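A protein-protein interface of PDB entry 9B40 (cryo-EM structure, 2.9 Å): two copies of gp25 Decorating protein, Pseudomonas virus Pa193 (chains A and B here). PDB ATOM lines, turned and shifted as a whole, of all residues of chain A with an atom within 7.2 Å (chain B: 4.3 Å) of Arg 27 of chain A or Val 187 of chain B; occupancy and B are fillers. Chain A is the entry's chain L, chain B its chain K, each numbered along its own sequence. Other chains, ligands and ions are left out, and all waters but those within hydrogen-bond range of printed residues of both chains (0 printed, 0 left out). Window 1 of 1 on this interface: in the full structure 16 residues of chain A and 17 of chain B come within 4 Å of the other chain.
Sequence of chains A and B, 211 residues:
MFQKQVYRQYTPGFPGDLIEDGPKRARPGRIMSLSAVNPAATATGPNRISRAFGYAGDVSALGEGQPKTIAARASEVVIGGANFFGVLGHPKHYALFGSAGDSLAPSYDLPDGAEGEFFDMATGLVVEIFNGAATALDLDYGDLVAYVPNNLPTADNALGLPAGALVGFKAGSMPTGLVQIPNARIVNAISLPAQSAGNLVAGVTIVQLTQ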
ATOM      1  N   ARG A  25       6.002 -14.848   9.749  1.00  0.00           N
ATOM      2  CA  ARG A  25       4.984 -14.593  10.762  1.00  0.00           C
ATOM      3  C   ARG A  25       5.147 -13.167  11.257  1.00  0.00           C
ATOM      4  O   ARG A  25       6.216 -12.805  11.757  1.00  0.00           O
ATOM      5  CB  ARG A  25       5.097 -15.572  11.934  1.00  0.00           C
ATOM      6  CG  ARG A  25       4.664 -16.988  11.619  1.00  0.00           C
ATOM      7  CD  ARG A  25       5.118 -17.942  12.704  1.00  0.00           C
ATOM      8  NE  ARG A  25       4.690 -19.309  12.443  1.00  0.00           N
ATOM      9  CZ  ARG A  25       4.977 -20.343  13.222  1.00  0.00           C
ATOM     10  NH1 ARG A  25       5.719 -20.204  14.306  1.00  0.00           N
ATOM     11  NH2 ARG A  25       4.512 -21.545  12.899  1.00  0.00           N
ATOM     12  N   ALA A  26       4.090 -12.368  11.119  1.00  0.00           N
ATOM     13  CA  ALA A  26       4.060 -11.007  11.627  1.00  0.00           C
ATOM     14  C   ALA A  26       2.732 -10.777  12.333  1.00  0.00           C
ATOM     15  O   ALA A  26       1.719 -11.393  11.995  1.00  0.00           O
ATOM     16  CB  ALA A  26       4.246  -9.977  10.506  1.00  0.00           C
ATOM     17  N   ARG A  27       2.746  -9.889  13.320  1.00  0.00           N
ATOM     18  CA  ARG A  27       1.546  -9.549  14.064  1.00  0.00           C
ATOM     19  C   ARG A  27       1.350  -8.042  14.063  1.00  0.00           C
ATOM     20  O   ARG A  27       2.325  -7.285  14.014  1.00  0.00           O
ATOM     21  CB  ARG A  27       1.623 -10.041  15.517  1.00  0.00           C
ATOM     22  CG  ARG A  27       0.577 -11.077  15.895  1.00  0.00           C
ATOM     23  CD  ARG A  27       0.926 -11.714  17.226  1.00  0.00           C
ATOM     24  NE  ARG A  27       2.069 -12.608  17.097  1.00  0.00           N
ATOM     25  CZ  ARG A  27       1.992 -13.882  16.745  1.00  0.00           C
ATOM     26  NH1 ARG A  27       0.829 -14.472  16.532  1.00  0.00           N
ATOM     27  NH2 ARG A  27       3.113 -14.581  16.600  1.00  0.00           N
ATOM     28  N   PRO A  28       0.108  -7.578  14.109  1.00  0.00           N
ATOM     29  CA  PRO A  28      -0.141  -6.147  14.284  1.00  0.00           C
ATOM     30  C   PRO A  28       0.083  -5.727  15.728  1.00  0.00           C
ATOM     31  O   PRO A  28      -0.015  -6.522  16.664  1.00  0.00           O
ATOM     32  CB  PRO A  28      -1.614  -5.982  13.885  1.00  0.00           C
ATOM     33  CG  PRO A  28      -2.032  -7.310  13.311  1.00  0.00           C
ATOM     34  CD  PRO A  28      -1.144  -8.326  13.923  1.00  0.00           C
ATOM     35  N   GLY A  29       0.390  -4.447  15.896  1.00  0.00           N
ATOM     36  CA  GLY A  29       0.612  -3.899  17.219  1.00  0.00           C
ATOM     37  C   GLY A  29       0.470  -2.398  17.203  1.00  0.00           C
ATOM     38  O   GLY A  29       0.646  -1.753  16.165  1.00  0.00           O
ATOM     39  N   TYR A  55       6.649  -6.426  23.823  1.00  0.00           N
ATOM     40  CA  TYR A  55       5.278  -6.507  24.305  1.00  0.00           C
ATOM     41  C   TYR A  55       5.119  -5.721  25.600  1.00  0.00           C
ATOM     42  O   TYR A  55       5.947  -5.815  26.508  1.00  0.00           O
ATOM     43  CB  TYR A  55       4.894  -7.969  24.525  1.00  0.00           C
ATOM     44  CG  TYR A  55       3.491  -8.189  25.032  1.00  0.00           C
ATOM     45  CD1 TYR A  55       2.394  -7.993  24.207  1.00  0.00           C
ATOM     46  CD2 TYR A  55       3.263  -8.601  26.338  1.00  0.00           C
ATOM     47  CE1 TYR A  55       1.111  -8.203  24.666  1.00  0.00           C
ATOM     48  CE2 TYR A  55       1.985  -8.811  26.805  1.00  0.00           C
ATOM     49  CZ  TYR A  55       0.913  -8.611  25.965  1.00  0.00           C
ATOM     50  OH  TYR A  55      -0.363  -8.818  26.432  1.00  0.00           O
ATOM     51  N   ARG A  73      -8.185  -8.855  18.833  1.00  0.00           N
ATOM     52  CA  ARG A  73      -7.000  -9.385  19.505  1.00  0.00           C
ATOM     53  C   ARG A  73      -5.831  -8.453  19.202  1.00  0.00           C
ATOM     54  O   ARG A  73      -4.979  -8.716  18.349  1.00  0.00           O
ATOM     55  CB  ARG A  73      -6.711 -10.814  19.068  1.00  0.00           C
ATOM     56  CG  ARG A  73      -7.468 -11.870  19.853  1.00  0.00           C
ATOM     57  CD  ARG A  73      -7.149 -13.290  19.389  1.00  0.00           C
ATOM     58  NE  ARG A  73      -5.732 -13.495  19.100  1.00  0.00           N
ATOM     59  CZ  ARG A  73      -5.215 -13.585  17.882  1.00  0.00           C
ATOM     60  NH1 ARG A  73      -5.973 -13.504  16.801  1.00  0.00           N
ATOM     61  NH2 ARG A  73      -3.903 -13.757  17.745  1.00  0.00           N
ATOM     62  N   SER A  75      -2.489  -6.083  20.413  1.00  0.00           N
ATOM     63  CA  SER A  75      -1.350  -6.052  21.315  1.00  0.00           C
ATOM     64  C   SER A  75      -0.748  -4.655  21.310  1.00  0.00           C
ATOM     65  O   SER A  75      -0.643  -4.019  20.258  1.00  0.00           O
ATOM     66  CB  SER A  75      -0.293  -7.081  20.909  1.00  0.00           C
ATOM     67  OG  SER A  75      -0.742  -8.398  21.163  1.00  0.00           O
ATOM     68  N   VAL A  77       2.608  -2.447  22.065  1.00  0.00           N
ATOM     69  CA  VAL A  77       4.040  -2.702  22.070  1.00  0.00           C
ATOM     70  C   VAL A  77       4.796  -1.407  22.328  1.00  0.00           C
ATOM     71  O   VAL A  77       4.296  -0.304  22.097  1.00  0.00           O
ATOM     72  CB  VAL A  77       4.525  -3.347  20.753  1.00  0.00           C
ATOM     73  CG1 VAL A  77       3.738  -4.608  20.456  1.00  0.00           C
ATOM     74  CG2 VAL A  77       4.404  -2.368  19.608  1.00  0.00           C
ATOM     75  N   PHE A  85       8.634  -8.736  20.906  1.00  0.00           N
ATOM     76  CA  PHE A  85       7.401  -8.933  20.158  1.00  0.00           C
ATOM     77  C   PHE A  85       7.657  -9.133  18.674  1.00  0.00           C
ATOM     78  O   PHE A  85       7.167 -10.098  18.085  1.00  0.00           O
ATOM     79  CB  PHE A  85       6.462  -7.735  20.370  1.00  0.00           C
ATOM     80  CG  PHE A  85       5.097  -7.912  19.764  1.00  0.00           C
ATOM     81  CD1 PHE A  85       4.092  -8.550  20.468  1.00  0.00           C
ATOM     82  CD2 PHE A  85       4.813  -7.421  18.500  1.00  0.00           C
ATOM     83  CE1 PHE A  85       2.836  -8.709  19.917  1.00  0.00           C
ATOM     84  CE2 PHE A  85       3.560  -7.579  17.946  1.00  0.00           C
ATOM     85  CZ  PHE A  85       2.571  -8.222  18.656  1.00  0.00           C
ATOM     86  N   GLY A  86       8.415  -8.240  18.056  1.00  0.00           N
ATOM     87  CA  GLY A  86       8.762  -8.397  16.657  1.00  0.00           C
ATOM     88  C   GLY A  86       9.570  -7.208  16.195  1.00  0.00           C
ATOM     89  O   GLY A  86       9.617  -6.163  16.851  1.00  0.00           O
ATOM     90  N   GLU A 115      -0.211   2.164  14.000  1.00  0.00           N
ATOM     91  CA  GLU A 115      -0.263   0.756  13.639  1.00  0.00           C
ATOM     92  C   GLU A 115       1.044   0.336  12.981  1.00  0.00           C
ATOM     93  O   GLU A 115       1.585   1.050  12.133  1.00  0.00           O
ATOM     94  CB  GLU A 115      -1.440   0.501  12.694  1.00  0.00           C
ATOM     95  CG  GLU A 115      -1.361  -0.765  11.850  1.00  0.00           C
ATOM     96  CD  GLU A 115      -1.794  -2.015  12.592  1.00  0.00           C
ATOM     97  OE1 GLU A 115      -1.962  -1.961  13.828  1.00  0.00           O
ATOM     98  OE2 GLU A 115      -1.974  -3.058  11.931  1.00  0.00           O
ATOM     99  N   GLY A 116       1.548  -0.825  13.375  1.00  0.00           N
ATOM    100  CA  GLY A 116       2.787  -1.337  12.820  1.00  0.00           C
ATOM    101  C   GLY A 116       2.705  -2.829  12.593  1.00  0.00           C
ATOM    102  O   GLY A 116       1.928  -3.536  13.238  1.00  0.00           O
ATOM    103  N   GLU A 117       3.520  -3.304  11.656  1.00  0.00           N
ATOM    104  CA  GLU A 117       3.622  -4.722  11.323  1.00  0.00           C
ATOM    105  C   GLU A 117       4.951  -5.234  11.861  1.00  0.00           C
ATOM    106  O   GLU A 117       6.011  -4.914  11.315  1.00  0.00           O
ATOM    107  CB  GLU A 117       3.527  -4.938   9.816  1.00  0.00           C
ATOM    108  CG  GLU A 117       2.242  -4.441   9.188  1.00  0.00           C
ATOM    109  CD  GLU A 117       2.154  -4.786   7.718  1.00  0.00           C
ATOM    110  OE1 GLU A 117       3.075  -5.459   7.212  1.00  0.00           O
ATOM    111  OE2 GLU A 117       1.169  -4.382   7.066  1.00  0.00           O
ATOM    112  N   PHE A 118       4.894  -6.042  12.911  1.00  0.00           N
ATOM    113  CA  PHE A 118       6.086  -6.507  13.610  1.00  0.00           C
ATOM    114  C   PHE A 118       6.302  -7.979  13.289  1.00  0.00           C
ATOM    115  O   PHE A 118       5.529  -8.838  13.725  1.00  0.00           O
ATOM    116  CB  PHE A 118       5.962  -6.266  15.111  1.00  0.00           C
ATOM    117  CG  PHE A 118       5.566  -4.861  15.458  1.00  0.00           C
ATOM    118  CD1 PHE A 118       6.530  -3.890  15.646  1.00  0.00           C
ATOM    119  CD2 PHE A 118       4.235  -4.509  15.591  1.00  0.00           C
ATOM    120  CE1 PHE A 118       6.175  -2.597  15.956  1.00  0.00           C
ATOM    121  CE2 PHE A 118       3.876  -3.215  15.897  1.00  0.00           C
ATOM    122  CZ  PHE A 118       4.847  -2.260  16.081  1.00  0.00           C
ATOM    123  N   PHE A 119       7.353  -8.260  12.525  1.00  0.00           N
ATOM    124  CA  PHE A 119       7.671  -9.614  12.109  1.00  0.00           C
ATOM    125  C   PHE A 119       8.273 -10.397  13.267  1.00  0.00           C
ATOM    126  O   PHE A 119       9.202  -9.924  13.931  1.00  0.00           O
ATOM    127  CB  PHE A 119       8.643  -9.594  10.931  1.00  0.00           C
ATOM    128  CG  PHE A 119       8.055  -9.040   9.666  1.00  0.00           C
ATOM    129  CD1 PHE A 119       8.004  -7.674   9.449  1.00  0.00           C
ATOM    130  CD2 PHE A 119       7.552  -9.885   8.694  1.00  0.00           C
ATOM    131  CE1 PHE A 119       7.466  -7.163   8.290  1.00  0.00           C
ATOM    132  CE2 PHE A 119       7.011  -9.380   7.532  1.00  0.00           C
ATOM    133  CZ  PHE A 119       6.968  -8.016   7.330  1.00  0.00           C
ATOM    134  N   ASP A 120       7.717 -11.584  13.513  1.00  0.00           N
ATOM    135  CA  ASP A 120       8.285 -12.568  14.425  1.00  0.00           C
ATOM    136  C   ASP A 120       9.171 -13.566  13.700  1.00  0.00           C
ATOM    137  O   ASP A 120      10.148 -14.055  14.277  1.00  0.00           O
ATOM    138  CB  ASP A 120       7.170 -13.334  15.140  1.00  0.00           C
ATOM    139  CG  ASP A 120       6.765 -12.694  16.447  1.00  0.00           C
ATOM    140  OD1 ASP A 120       7.453 -12.930  17.462  1.00  0.00           O
ATOM    141  OD2 ASP A 120       5.752 -11.963  16.460  1.00  0.00           O
ATOM    142  N   MET A 121       8.831 -13.885  12.455  1.00  0.00           N
ATOM    143  CA  MET A 121       9.594 -14.802  11.624  1.00  0.00           C
ATOM    144  C   MET A 121       9.664 -14.227  10.219  1.00  0.00           C
ATOM    145  O   MET A 121       8.661 -13.741   9.691  1.00  0.00           O
ATOM    146  CB  MET A 121       8.953 -16.200  11.612  1.00  0.00           C
ATOM    147  CG  MET A 121       9.251 -17.025  10.373  1.00  0.00           C
ATOM    148  SD  MET A 121       8.611 -18.710  10.413  1.00  0.00           S
ATOM    149  CE  MET A 121       8.766 -19.092  12.151  1.00  0.00           C
ATOM    150  N   GLN A 211      13.903 -16.340  13.246  1.00  0.00           N
ATOM    151  CA  GLN A 211      13.389 -17.696  13.466  1.00  0.00           C
ATOM    152  C   GLN A 211      13.530 -18.597  12.245  1.00  0.00           C
ATOM    153  O   GLN A 211      13.036 -19.724  12.238  1.00  0.00           O
ATOM    154  CB  GLN A 211      11.926 -17.659  13.909  1.00  0.00           C
ATOM    155  CG  GLN A 211      11.736 -17.895  15.392  1.00  0.00           C
ATOM    156  CD  GLN A 211      10.335 -17.568  15.855  1.00  0.00           C
ATOM    157  OE1 GLN A 211       9.375 -17.702  15.101  1.00  0.00           O
ATOM    158  NE2 GLN A 211      10.212 -17.135  17.104  1.00  0.00           N
ATOM    159  N   GLU B  20      -4.569 -18.309  13.628  1.00  0.00           N
ATOM    160  CA  GLU B  20      -3.769 -17.577  12.662  1.00  0.00           C
ATOM    161  C   GLU B  20      -3.255 -18.496  11.564  1.00  0.00           C
ATOM    162  O   GLU B  20      -2.853 -19.633  11.820  1.00  0.00           O
ATOM    163  CB  GLU B  20      -2.614 -16.854  13.348  1.00  0.00           C
ATOM    164  CG  GLU B  20      -2.945 -16.408  14.753  1.00  0.00           C
ATOM    165  CD  GLU B  20      -2.174 -15.175  15.157  1.00  0.00           C
ATOM    166  OE1 GLU B  20      -0.950 -15.284  15.353  1.00  0.00           O
ATOM    167  OE2 GLU B  20      -2.791 -14.096  15.276  1.00  0.00           O
ATOM    168  N   TYR B 141       2.915 -12.722  26.764  1.00  0.00           N
ATOM    169  CA  TYR B 141       3.439 -13.007  25.431  1.00  0.00           C
ATOM    170  C   TYR B 141       4.697 -13.866  25.494  1.00  0.00           C
ATOM    171  O   TYR B 141       4.878 -14.779  24.680  1.00  0.00           O
ATOM    172  CB  TYR B 141       3.725 -11.697  24.699  1.00  0.00           C
ATOM    173  CG  TYR B 141       3.755 -11.816  23.196  1.00  0.00           C
ATOM    174  CD1 TYR B 141       2.590 -12.021  22.477  1.00  0.00           C
ATOM    175  CD2 TYR B 141       4.949 -11.724  22.497  1.00  0.00           C
ATOM    176  CE1 TYR B 141       2.608 -12.133  21.106  1.00  0.00           C
ATOM    177  CE2 TYR B 141       4.977 -11.833  21.122  1.00  0.00           C
ATOM    178  CZ  TYR B 141       3.802 -12.038  20.432  1.00  0.00           C
ATOM    179  OH  TYR B 141       3.820 -12.148  19.061  1.00  0.00           O
ATOM    180  N   ARG B 185       5.364 -20.980  22.465  1.00  0.00           N
ATOM    181  CA  ARG B 185       5.150 -19.693  23.109  1.00  0.00           C
ATOM    182  C   ARG B 185       3.666 -19.439  23.330  1.00  0.00           C
ATOM    183  O   ARG B 185       2.834 -19.782  22.487  1.00  0.00           O
ATOM    184  CB  ARG B 185       5.755 -18.561  22.275  1.00  0.00           C
ATOM    185  CG  ARG B 185       7.001 -17.961  22.891  1.00  0.00           C
ATOM    186  CD  ARG B 185       7.895 -17.315  21.848  1.00  0.00           C
ATOM    187  NE  ARG B 185       7.461 -15.975  21.476  1.00  0.00           N
ATOM    188  CZ  ARG B 185       6.973 -15.655  20.287  1.00  0.00           C
ATOM    189  NH1 ARG B 185       6.848 -16.555  19.327  1.00  0.00           N
ATOM    190  NH2 ARG B 185       6.614 -14.397  20.048  1.00  0.00           N
ATOM    191  N   ILE B 186       3.350 -18.825  24.464  1.00  0.00           N
ATOM    192  CA  ILE B 186       1.995 -18.384  24.774  1.00  0.00           C
ATOM    193  C   ILE B 186       1.810 -17.008  24.148  1.00  0.00           C
ATOM    194  O   ILE B 186       2.405 -16.029  24.601  1.00  0.00           O
ATOM    195  CB  ILE B 186       1.753 -18.341  26.288  1.00  0.00           C
ATOM    196  CG1 ILE B 186       2.173 -19.656  26.952  1.00  0.00           C
ATOM    197  CG2 ILE B 186       0.315 -18.005  26.589  1.00  0.00           C
ATOM    198  CD1 ILE B 186       1.072 -20.692  27.031  1.00  0.00           C
ATOM    199  N   VAL B 187       0.985 -16.926  23.108  1.00  0.00           N
ATOM    200  CA  VAL B 187       0.819 -15.661  22.394  1.00  0.00           C
ATOM    201  C   VAL B 187      -0.123 -14.735  23.153  1.00  0.00           C
ATOM    202  O   VAL B 187       0.267 -13.650  23.593  1.00  0.00           O
ATOM    203  CB  VAL B 187       0.334 -15.916  20.956  1.00  0.00           C
ATOM    204  CG1 VAL B 187      -0.179 -14.631  20.325  1.00  0.00           C
ATOM    205  CG2 VAL B 187       1.454 -16.502  20.125  1.00  0.00           C
ATOM    206  N   ASN B 188      -1.372 -15.150  23.330  1.00  0.00           N
ATOM    207  CA  ASN B 188      -2.302 -14.325  24.082  1.00  0.00           C
ATOM    208  C   ASN B 188      -1.995 -14.423  25.574  1.00  0.00           C
ATOM    209  O   ASN B 188      -1.383 -15.380  26.047  1.00  0.00           O
ATOM    210  CB  ASN B 188      -3.743 -14.743  23.788  1.00  0.00           C
ATOM    211  CG  ASN B 188      -4.688 -13.567  23.710  1.00  0.00           C
ATOM    212  OD1 ASN B 188      -4.268 -12.429  23.508  1.00  0.00           O
ATOM    213  ND2 ASN B 188      -5.976 -13.834  23.879  1.00  0.00           N
ATOM    214  N   ALA B 189      -2.415 -13.407  26.320  1.00  0.00           N
ATOM    215  CA  ALA B 189      -2.130 -13.310  27.745  1.00  0.00           C
ATOM    216  C   ALA B 189      -3.393 -13.583  28.547  1.00  0.00           C
ATOM    217  O   ALA B 189      -4.466 -13.074  28.215  1.00  0.00           O
ATOM    218  CB  ALA B 189      -1.576 -11.928  28.098  1.00  0.00           C
ATOM    219  N   VAL B 207      -4.272 -18.927  22.794  1.00  0.00           N
ATOM    220  CA  VAL B 207      -3.565 -18.973  21.521  1.00  0.00           C
ATOM    221  C   VAL B 207      -2.092 -19.226  21.804  1.00  0.00           C
ATOM    222  O   VAL B 207      -1.484 -18.555  22.645  1.00  0.00           O
ATOM    223  CB  VAL B 207      -3.764 -17.669  20.733  1.00  0.00           C
ATOM    224  CG1 VAL B 207      -3.070 -17.757  19.387  1.00  0.00           C
ATOM    225  CG2 VAL B 207      -5.237 -17.379  20.546  1.00  0.00           C
ATOM    226  N   GLN B 208      -1.518 -20.203  21.115  1.00  0.00           N
ATOM    227  CA  GLN B 208      -0.118 -20.544  21.285  1.00  0.00           C
ATOM    228  C   GLN B 208       0.546 -20.653  19.920  1.00  0.00           C
ATOM    229  O   GLN B 208      -0.094 -20.996  18.920  1.00  0.00           O
ATOM    230  CB  GLN B 208       0.044 -21.851  22.083  1.00  0.00           C
ATOM    231  CG  GLN B 208       0.264 -23.095  21.246  1.00  0.00           C
ATOM    232  CD  GLN B 208       0.881 -24.226  22.036  1.00  0.00           C
ATOM    233  OE1 GLN B 208       1.044 -24.131  23.249  1.00  0.00           O
ATOM    234  NE2 GLN B 208       1.227 -25.309  21.349  1.00  0.00           N
ATOM    235  N   LEU B 209       1.829 -20.313  19.886  1.00  0.00           N
ATOM    236  CA  LEU B 209       2.653 -20.433  18.692  1.00  0.00           C
ATOM    237  C   LEU B 209       3.680 -21.521  18.952  1.00  0.00           C
ATOM    238  O   LEU B 209       4.429 -21.449  19.932  1.00  0.00           O
ATOM    239  CB  LEU B 209       3.327 -19.103  18.348  1.00  0.00           C
ATOM    240  CG  LEU B 209       4.294 -19.035  17.161  1.00  0.00           C
ATOM    241  CD1 LEU B 209       4.132 -17.711  16.460  1.00  0.00           C
ATOM    242  CD2 LEU B 209       5.746 -19.202  17.584  1.00  0.00           C
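The side-chain carboxylate (OE2) of Glu 20 of chain B lies within salt-bridge range of the guanidinium group (NH1) of Arg 27 of chain A (3.9 Å). The side-chain carboxylate (OE2) of Glu 20 of chain B is in salt-bridge range of the guanidinium group (NH2) of Arg 73 of chain A (2.7 Å). The side-chain hydroxyl of Tyr 141 of chain B lies within hydrogen-bond range of the guanidinium group of Arg 27 of chain A (2.7 Å). The side-chain hydroxyl of Tyr 141 of chain B sits at hydrogen-bond distance from the side-chain carboxylate of Asp 120 of chain A. The guanidinium group (NH2) of Arg 185 of chain B is in salt-bridge range of the side-chain carboxylate (OD1) of Asp 120 of chain A (3.1 Å).
The backbone NH (N) of Arg 185 of chain B lies within hydrogen-bond range of the backbone carbonyl oxygen (O) of Leu 209 of chain B, 2.7 Å away. N of Val 187 of chain B is in hydrogen-bond range of O of Val 207 of chain B, at 3.0 Å. The backbone carbonyl oxygen (O) of Arg 25 of chain A sits at hydrogen-bond distance from the backbone NH (N) of Asp 120 of chain A (2.6 Å). The backbone NH (N) of Arg 25 of chain A lies within hydrogen-bond range of the backbone carbonyl oxygen (O) of Met 121 of chain A (2.9 Å). N of Arg 27 of chain A is in hydrogen-bond range of O of Phe 118 of chain A. NH2 of Arg 27 of chain A lies within salt-bridge range of OD2 of Asp 120 of chain A (3.7 Å).
Among the printed residues, merely in contact across the chains: Arg 25 of chain A with Leu 209 of chain B (3.4 Å), Arg 27 of chain A with Val 187 of chain B (3.9 Å), Arg 27 of chain A with Leu 209 of chain B (3.3 Å), Tyr 55 of chain A with Tyr 141 of chain B (3.5 Å), Tyr 55 of chain A with Ala 189 of chain B (3.7 Å) and Phe 85 of chain A with Tyr 141 of chain B (3.5 Å).
Of the printed residues of chain B, Arg 73 of chain A touches Glu 20 (2.7 Å). Ser 75 of chain A touches none of the printed residues of chain B. Phe 118 of chain A touches none of the printed residues of chain B. Of the printed residues of chain A, Leu 209 of chain B touches Arg 25 (3.4 Å) and Arg 27 (3.3 Å). The nearest printed residue of chain A that does not touch Glu 20 of chain B is Ala 26 of chain A (5.8 Å).
Of the 10 printed residues of chain B, 6 touch a printed residue of chain A. Among the printed residues, Asp or Glu carboxylates within 4 Å of a Lys or Arg side-chain nitrogen of the other chain: Arg 27 of chain A with Glu 20 of chain B, Arg 73 of chain A with Glu 20 of chain B and Asp 120 of chain A with Arg 185 of chain B.
No position is printed for both chains. Of the 11 pairs that touch across the chains among the printed residues, none has its exchanged pair printed and touching as well.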
